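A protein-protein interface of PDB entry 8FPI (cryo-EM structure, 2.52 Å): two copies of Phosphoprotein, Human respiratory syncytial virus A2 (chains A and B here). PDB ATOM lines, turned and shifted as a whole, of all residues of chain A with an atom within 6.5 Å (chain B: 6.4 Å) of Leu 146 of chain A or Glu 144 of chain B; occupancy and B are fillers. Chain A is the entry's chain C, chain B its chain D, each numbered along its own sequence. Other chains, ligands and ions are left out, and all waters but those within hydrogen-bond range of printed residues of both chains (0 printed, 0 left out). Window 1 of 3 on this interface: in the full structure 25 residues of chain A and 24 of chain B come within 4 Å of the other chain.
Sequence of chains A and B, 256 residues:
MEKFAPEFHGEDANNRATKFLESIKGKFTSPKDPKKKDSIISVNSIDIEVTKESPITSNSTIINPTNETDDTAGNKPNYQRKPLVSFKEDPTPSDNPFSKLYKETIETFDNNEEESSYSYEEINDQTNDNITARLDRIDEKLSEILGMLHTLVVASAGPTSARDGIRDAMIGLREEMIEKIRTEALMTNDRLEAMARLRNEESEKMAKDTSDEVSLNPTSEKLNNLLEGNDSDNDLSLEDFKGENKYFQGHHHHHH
The side-chain amino group (NZ) of Lys 141 of chain B is in hydrogen-bond range of the side-chain hydroxyl (OG) of Ser 143 of chain A.
Printed residues of chain A that touch a printed residue of chain B: Leu 142, Ser 143, Ile 145, Leu 146, Leu 149 and His 150.
Hydrophobic or aromatic side chains of chain A that line the printed part of chain B: Leu 142, Ile 145, Leu 146, Leu 149 and His 150.
Hydrophobic or aromatic side chains of chain B that line the printed part of chain A: Leu 142, Ile 145, Met 148 and Leu 149.
Among the printed residues, no Asp or Glu carboxylate lies within 4 Å of a Lys or Arg side-chain nitrogen of the other chain.
Leu 142 of chain A touches Lys 141 of chain B, but with the chains exchanged Lys 141 of chain A does not touch Leu 142 of chain B (9.4 Å).
Leu 142 of chain B touches its own counterpart, Leu 142 of chain A.
Leu 146 of chain A touches Lys 141 of chain B, but with the chains exchanged Lys 141 of chain A does not touch Leu 146 of chain B (11.8 Å).
Leu 149 of chain A touches Met 148 of chain B, but with the chains exchanged Met 148 of chain A does not touch Leu 149 of chain B (8.7 Å).
Of the 13 pairs that touch across the chains among the printed residues, 3 have their exchanged pair printed and touching as well.
Among the printed residues, pairs that only touch across the chains: Leu 142 of chain A with Lys 141 of chain B, Leu 142 of chain A with Leu 142 of chain B, Leu 142 of chain A with Ile 145 of chain B, Ile 145 of chain A with Ile 145 of chain B, Leu 146 of chain A with Lys 141 of chain B, Leu 146 of chain A with Glu 144 of chain B, Leu 146 of chain A with Ile 145 of chain B, Leu 146 of chain A with Met 148 of chain B, Leu 149 of chain A with Ile 145 of chain B, Leu 149 of chain A with Met 148 of chain B, Leu 149 of chain A with Leu 149 of chain B and His 150 of chain A with Met 148 of chain B.
Leu 146 of chain A touches just these residues of chain B: Lys 141, Glu 144, Ile 145 and Met 148.
Glu 144 of chain B touches just one residue of chain A: Leu 146 (3.3 Å).
Printed residues of chain B within 4 Å of Ile 145 of chain A: Ile 145.
Of the printed residues of chain A, Lys 141 of chain B touches Leu 142, Ser 143 and Leu 146.
Printed residues of chain A within 4 Å of Leu 149 of chain B: Leu 149 (3.3 Å).
Of the printed residues of chain A, Leu 142 of chain B touches Leu 142 (3.8 Å).
Of the printed residues of chain A, Met 148 of chain B touches Leu 146 (3.4 Å), Leu 149 (3.1 Å) and His 150 (2.9 Å).
Glu 144 of chain A touches none of the printed residues of chain B.
The nearest residue of chain B that does not touch Leu 146 of chain A is Leu 142 of chain B (5.7 Å).
The nearest printed residue of chain A that does not touch Glu 144 of chain B is Leu 149 of chain A (6.7 Å).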
ATOM      1  N   LYS A 141     -26.428 -19.306 -11.751  1.00  0.00           N
ATOM      2  CA  LYS A 141     -26.403 -20.722 -11.415  1.00  0.00           C
ATOM      3  C   LYS A 141     -25.183 -21.088 -10.584  1.00  0.00           C
ATOM      4  O   LYS A 141     -25.281 -21.893  -9.654  1.00  0.00           O
ATOM      5  CB  LYS A 141     -26.440 -21.569 -12.687  1.00  0.00           C
ATOM      6  CG  LYS A 141     -27.786 -21.604 -13.383  1.00  0.00           C
ATOM      7  CD  LYS A 141     -27.838 -22.722 -14.405  1.00  0.00           C
ATOM      8  CE  LYS A 141     -28.972 -22.524 -15.388  1.00  0.00           C
ATOM      9  NZ  LYS A 141     -28.562 -21.683 -16.542  1.00  0.00           N
ATOM     10  N   LEU A 142     -24.028 -20.513 -10.903  1.00  0.00           N
ATOM     11  CA  LEU A 142     -22.832 -20.750 -10.120  1.00  0.00           C
ATOM     12  C   LEU A 142     -22.945 -20.168  -8.720  1.00  0.00           C
ATOM     13  O   LEU A 142     -22.189 -20.576  -7.837  1.00  0.00           O
ATOM     14  CB  LEU A 142     -21.638 -20.165 -10.872  1.00  0.00           C
ATOM     15  CG  LEU A 142     -20.237 -20.653 -10.528  1.00  0.00           C
ATOM     16  CD1 LEU A 142     -19.949 -21.976 -11.182  1.00  0.00           C
ATOM     17  CD2 LEU A 142     -19.245 -19.636 -11.002  1.00  0.00           C
ATOM     18  N   SER A 143     -23.867 -19.231  -8.499  1.00  0.00           N
ATOM     19  CA  SER A 143     -24.195 -18.759  -7.160  1.00  0.00           C
ATOM     20  C   SER A 143     -25.040 -19.772  -6.393  1.00  0.00           C
ATOM     21  O   SER A 143     -24.851 -19.972  -5.186  1.00  0.00           O
ATOM     22  CB  SER A 143     -24.938 -17.426  -7.253  1.00  0.00           C
ATOM     23  OG  SER A 143     -24.157 -16.461  -7.925  1.00  0.00           O
ATOM     24  N   GLU A 144     -25.992 -20.407  -7.080  1.00  0.00           N
ATOM     25  CA  GLU A 144     -26.797 -21.451  -6.460  1.00  0.00           C
ATOM     26  C   GLU A 144     -25.939 -22.645  -6.072  1.00  0.00           C
ATOM     27  O   GLU A 144     -26.140 -23.245  -5.010  1.00  0.00           O
ATOM     28  CB  GLU A 144     -27.915 -21.863  -7.418  1.00  0.00           C
ATOM     29  CG  GLU A 144     -28.846 -22.920  -6.890  1.00  0.00           C
ATOM     30  CD  GLU A 144     -30.238 -22.824  -7.482  1.00  0.00           C
ATOM     31  OE1 GLU A 144     -30.742 -21.692  -7.629  1.00  0.00           O
ATOM     32  OE2 GLU A 144     -30.834 -23.879  -7.792  1.00  0.00           O
ATOM     33  N   ILE A 145     -24.972 -22.996  -6.916  1.00  0.00           N
ATOM     34  CA  ILE A 145     -24.029 -24.042  -6.545  1.00  0.00           C
ATOM     35  C   ILE A 145     -23.302 -23.667  -5.264  1.00  0.00           C
ATOM     36  O   ILE A 145     -23.055 -24.522  -4.404  1.00  0.00           O
ATOM     37  CB  ILE A 145     -23.032 -24.302  -7.682  1.00  0.00           C
ATOM     38  CG1 ILE A 145     -23.728 -24.968  -8.860  1.00  0.00           C
ATOM     39  CG2 ILE A 145     -21.912 -25.181  -7.196  1.00  0.00           C
ATOM     40  CD1 ILE A 145     -22.950 -24.892 -10.142  1.00  0.00           C
ATOM     41  N   LEU A 146     -22.925 -22.397  -5.121  1.00  0.00           N
ATOM     42  CA  LEU A 146     -22.238 -21.951  -3.914  1.00  0.00           C
ATOM     43  C   LEU A 146     -23.125 -22.097  -2.691  1.00  0.00           C
ATOM     44  O   LEU A 146     -22.673 -22.547  -1.635  1.00  0.00           O
ATOM     45  CB  LEU A 146     -21.804 -20.499  -4.073  1.00  0.00           C
ATOM     46  CG  LEU A 146     -20.483 -20.277  -4.791  1.00  0.00           C
ATOM     47  CD1 LEU A 146     -20.411 -18.840  -5.180  1.00  0.00           C
ATOM     48  CD2 LEU A 146     -19.317 -20.661  -3.915  1.00  0.00           C
ATOM     49  N   GLY A 147     -24.382 -21.688  -2.808  1.00  0.00           N
ATOM     50  CA  GLY A 147     -25.305 -21.870  -1.703  1.00  0.00           C
ATOM     51  C   GLY A 147     -25.434 -23.321  -1.286  1.00  0.00           C
ATOM     52  O   GLY A 147     -25.365 -23.644  -0.092  1.00  0.00           O
ATOM     53  N   MET A 148     -25.602 -24.217  -2.261  1.00  0.00           N
ATOM     54  CA  MET A 148     -25.655 -25.651  -1.987  1.00  0.00           C
ATOM     55  C   MET A 148     -24.427 -26.081  -1.199  1.00  0.00           C
ATOM     56  O   MET A 148     -24.531 -26.567  -0.070  1.00  0.00           O
ATOM     57  CB  MET A 148     -25.728 -26.436  -3.301  1.00  0.00           C
ATOM     58  CG  MET A 148     -26.915 -26.122  -4.197  1.00  0.00           C
ATOM     59  SD  MET A 148     -28.285 -27.263  -4.032  1.00  0.00           S
ATOM     60  CE  MET A 148     -29.168 -26.534  -2.680  1.00  0.00           C
ATOM     61  N   LEU A 149     -23.251 -25.892  -1.793  1.00  0.00           N
ATOM     62  CA  LEU A 149     -22.039 -26.446  -1.214  1.00  0.00           C
ATOM     63  C   LEU A 149     -21.694 -25.800   0.113  1.00  0.00           C
ATOM     64  O   LEU A 149     -20.995 -26.407   0.929  1.00  0.00           O
ATOM     65  CB  LEU A 149     -20.879 -26.298  -2.180  1.00  0.00           C
ATOM     66  CG  LEU A 149     -20.912 -27.331  -3.296  1.00  0.00           C
ATOM     67  CD1 LEU A 149     -20.632 -26.663  -4.611  1.00  0.00           C
ATOM     68  CD2 LEU A 149     -19.923 -28.456  -3.036  1.00  0.00           C
ATOM     69  N   HIS A 150     -22.157 -24.574   0.354  1.00  0.00           N
ATOM     70  CA  HIS A 150     -21.923 -23.959   1.654  1.00  0.00           C
ATOM     71  C   HIS A 150     -22.803 -24.601   2.709  1.00  0.00           C
ATOM     72  O   HIS A 150     -22.311 -25.074   3.739  1.00  0.00           O
ATOM     73  CB  HIS A 150     -22.183 -22.457   1.608  1.00  0.00           C
ATOM     74  CG  HIS A 150     -21.899 -21.773   2.907  1.00  0.00           C
ATOM     75  ND1 HIS A 150     -22.832 -21.003   3.566  1.00  0.00           N
ATOM     76  CD2 HIS A 150     -20.790 -21.767   3.684  1.00  0.00           C
ATOM     77  CE1 HIS A 150     -22.306 -20.547   4.686  1.00  0.00           C
ATOM     78  NE2 HIS A 150     -21.070 -20.997   4.783  1.00  0.00           N
ATOM     79  N   THR A 151     -24.114 -24.644   2.460  1.00  0.00           N
ATOM     80  CA  THR A 151     -24.988 -25.296   3.420  1.00  0.00           C
ATOM     81  C   THR A 151     -24.541 -26.721   3.689  1.00  0.00           C
ATOM     82  O   THR A 151     -24.796 -27.247   4.773  1.00  0.00           O
ATOM     83  CB  THR A 151     -26.420 -25.304   2.923  1.00  0.00           C
ATOM     84  OG1 THR A 151     -26.843 -23.967   2.672  1.00  0.00           O
ATOM     85  CG2 THR A 151     -27.309 -25.920   3.953  1.00  0.00           C
ATOM     86  N   ASP B 139     -14.597 -16.383 -12.180  1.00  0.00           N
ATOM     87  CA  ASP B 139     -13.414 -17.082 -11.697  1.00  0.00           C
ATOM     88  C   ASP B 139     -13.238 -16.958 -10.191  1.00  0.00           C
ATOM     89  O   ASP B 139     -12.639 -17.847  -9.577  1.00  0.00           O
ATOM     90  CB  ASP B 139     -12.165 -16.569 -12.400  1.00  0.00           C
ATOM     91  CG  ASP B 139     -12.219 -16.768 -13.895  1.00  0.00           C
ATOM     92  OD1 ASP B 139     -12.196 -17.932 -14.344  1.00  0.00           O
ATOM     93  OD2 ASP B 139     -12.249 -15.763 -14.624  1.00  0.00           O
ATOM     94  N   GLU B 140     -13.723 -15.879  -9.585  1.00  0.00           N
ATOM     95  CA  GLU B 140     -13.683 -15.724  -8.140  1.00  0.00           C
ATOM     96  C   GLU B 140     -14.871 -16.378  -7.460  1.00  0.00           C
ATOM     97  O   GLU B 140     -14.756 -16.802  -6.308  1.00  0.00           O
ATOM     98  CB  GLU B 140     -13.630 -14.240  -7.766  1.00  0.00           C
ATOM     99  CG  GLU B 140     -12.744 -13.926  -6.573  1.00  0.00           C
ATOM    100  CD  GLU B 140     -11.309 -14.370  -6.774  1.00  0.00           C
ATOM    101  OE1 GLU B 140     -10.834 -15.219  -5.992  1.00  0.00           O
ATOM    102  OE2 GLU B 140     -10.661 -13.872  -7.718  1.00  0.00           O
ATOM    103  N   LYS B 141     -16.005 -16.470  -8.143  1.00  0.00           N
ATOM    104  CA  LYS B 141     -17.124 -17.276  -7.690  1.00  0.00           C
ATOM    105  C   LYS B 141     -16.886 -18.759  -7.895  1.00  0.00           C
ATOM    106  O   LYS B 141     -17.413 -19.571  -7.131  1.00  0.00           O
ATOM    107  CB  LYS B 141     -18.382 -16.870  -8.451  1.00  0.00           C
ATOM    108  CG  LYS B 141     -19.650 -17.204  -7.761  1.00  0.00           C
ATOM    109  CD  LYS B 141     -20.796 -16.676  -8.550  1.00  0.00           C
ATOM    110  CE  LYS B 141     -20.906 -15.188  -8.403  1.00  0.00           C
ATOM    111  NZ  LYS B 141     -22.316 -14.731  -8.458  1.00  0.00           N
ATOM    112  N   LEU B 142     -16.101 -19.116  -8.903  1.00  0.00           N
ATOM    113  CA  LEU B 142     -15.776 -20.491  -9.229  1.00  0.00           C
ATOM    114  C   LEU B 142     -14.575 -20.987  -8.436  1.00  0.00           C
ATOM    115  O   LEU B 142     -14.304 -22.186  -8.423  1.00  0.00           O
ATOM    116  CB  LEU B 142     -15.528 -20.588 -10.736  1.00  0.00           C
ATOM    117  CG  LEU B 142     -15.599 -21.907 -11.493  1.00  0.00           C
ATOM    118  CD1 LEU B 142     -15.430 -21.621 -12.966  1.00  0.00           C
ATOM    119  CD2 LEU B 142     -14.560 -22.892 -11.047  1.00  0.00           C
ATOM    120  N   SER B 143     -13.861 -20.090  -7.758  1.00  0.00           N
ATOM    121  CA  SER B 143     -12.833 -20.478  -6.808  1.00  0.00           C
ATOM    122  C   SER B 143     -13.361 -20.607  -5.390  1.00  0.00           C
ATOM    123  O   SER B 143     -12.732 -21.291  -4.576  1.00  0.00           O
ATOM    124  CB  SER B 143     -11.677 -19.470  -6.815  1.00  0.00           C
ATOM    125  OG  SER B 143     -10.462 -20.104  -6.462  1.00  0.00           O
ATOM    126  N   GLU B 144     -14.485 -19.970  -5.071  1.00  0.00           N
ATOM    127  CA  GLU B 144     -15.172 -20.276  -3.826  1.00  0.00           C
ATOM    128  C   GLU B 144     -15.664 -21.715  -3.832  1.00  0.00           C
ATOM    129  O   GLU B 144     -15.458 -22.456  -2.867  1.00  0.00           O
ATOM    130  CB  GLU B 144     -16.336 -19.309  -3.626  1.00  0.00           C
ATOM    131  CG  GLU B 144     -15.943 -17.962  -3.064  1.00  0.00           C
ATOM    132  CD  GLU B 144     -16.090 -17.883  -1.559  1.00  0.00           C
ATOM    133  OE1 GLU B 144     -17.063 -18.451  -1.023  1.00  0.00           O
ATOM    134  OE2 GLU B 144     -15.233 -17.248  -0.910  1.00  0.00           O
ATOM    135  N   ILE B 145     -16.289 -22.139  -4.936  1.00  0.00           N
ATOM    136  CA  ILE B 145     -16.798 -23.501  -5.048  1.00  0.00           C
ATOM    137  C   ILE B 145     -15.691 -24.520  -4.885  1.00  0.00           C
ATOM    138  O   ILE B 145     -15.886 -25.551  -4.239  1.00  0.00           O
ATOM    139  CB  ILE B 145     -17.497 -23.703  -6.404  1.00  0.00           C
ATOM    140  CG1 ILE B 145     -18.775 -22.888  -6.471  1.00  0.00           C
ATOM    141  CG2 ILE B 145     -17.801 -25.163  -6.621  1.00  0.00           C
ATOM    142  CD1 ILE B 145     -19.267 -22.681  -7.864  1.00  0.00           C
ATOM    143  N   LEU B 146     -14.531 -24.264  -5.467  1.00  0.00           N
ATOM    144  CA  LEU B 146     -13.417 -25.187  -5.402  1.00  0.00           C
ATOM    145  C   LEU B 146     -12.722 -25.174  -4.051  1.00  0.00           C
ATOM    146  O   LEU B 146     -11.863 -26.020  -3.805  1.00  0.00           O
ATOM    147  CB  LEU B 146     -12.411 -24.858  -6.504  1.00  0.00           C
ATOM    148  CG  LEU B 146     -11.499 -25.965  -7.037  1.00  0.00           C
ATOM    149  CD1 LEU B 146     -12.108 -27.355  -6.956  1.00  0.00           C
ATOM    150  CD2 LEU B 146     -11.133 -25.633  -8.465  1.00  0.00           C
ATOM    151  N   GLY B 147     -13.065 -24.239  -3.174  1.00  0.00           N
ATOM    152  CA  GLY B 147     -12.497 -24.216  -1.843  1.00  0.00           C
ATOM    153  C   GLY B 147     -13.438 -24.858  -0.852  1.00  0.00           C
ATOM    154  O   GLY B 147     -13.013 -25.407   0.166  1.00  0.00           O
ATOM    155  N   MET B 148     -14.730 -24.790  -1.154  1.00  0.00           N
ATOM    156  CA  MET B 148     -15.745 -25.474  -0.373  1.00  0.00           C
ATOM    157  C   MET B 148     -15.904 -26.932  -0.760  1.00  0.00           C
ATOM    158  O   MET B 148     -16.638 -27.656  -0.083  1.00  0.00           O
ATOM    159  CB  MET B 148     -17.077 -24.749  -0.521  1.00  0.00           C
ATOM    160  CG  MET B 148     -16.949 -23.284  -0.196  1.00  0.00           C
ATOM    161  SD  MET B 148     -18.462 -22.333  -0.138  1.00  0.00           S
ATOM    162  CE  MET B 148     -19.629 -23.552  -0.648  1.00  0.00           C
ATOM    163  N   LEU B 149     -15.247 -27.381  -1.824  1.00  0.00           N
ATOM    164  CA  LEU B 149     -15.189 -28.797  -2.131  1.00  0.00           C
ATOM    165  C   LEU B 149     -13.969 -29.467  -1.529  1.00  0.00           C
ATOM    166  O   LEU B 149     -14.004 -30.674  -1.281  1.00  0.00           O
ATOM    167  CB  LEU B 149     -15.196 -29.013  -3.646  1.00  0.00           C
ATOM    168  CG  LEU B 149     -16.578 -28.940  -4.295  1.00  0.00           C
ATOM    169  CD1 LEU B 149     -16.472 -28.673  -5.777  1.00  0.00           C
ATOM    170  CD2 LEU B 149     -17.353 -30.208  -4.041  1.00  0.00           C
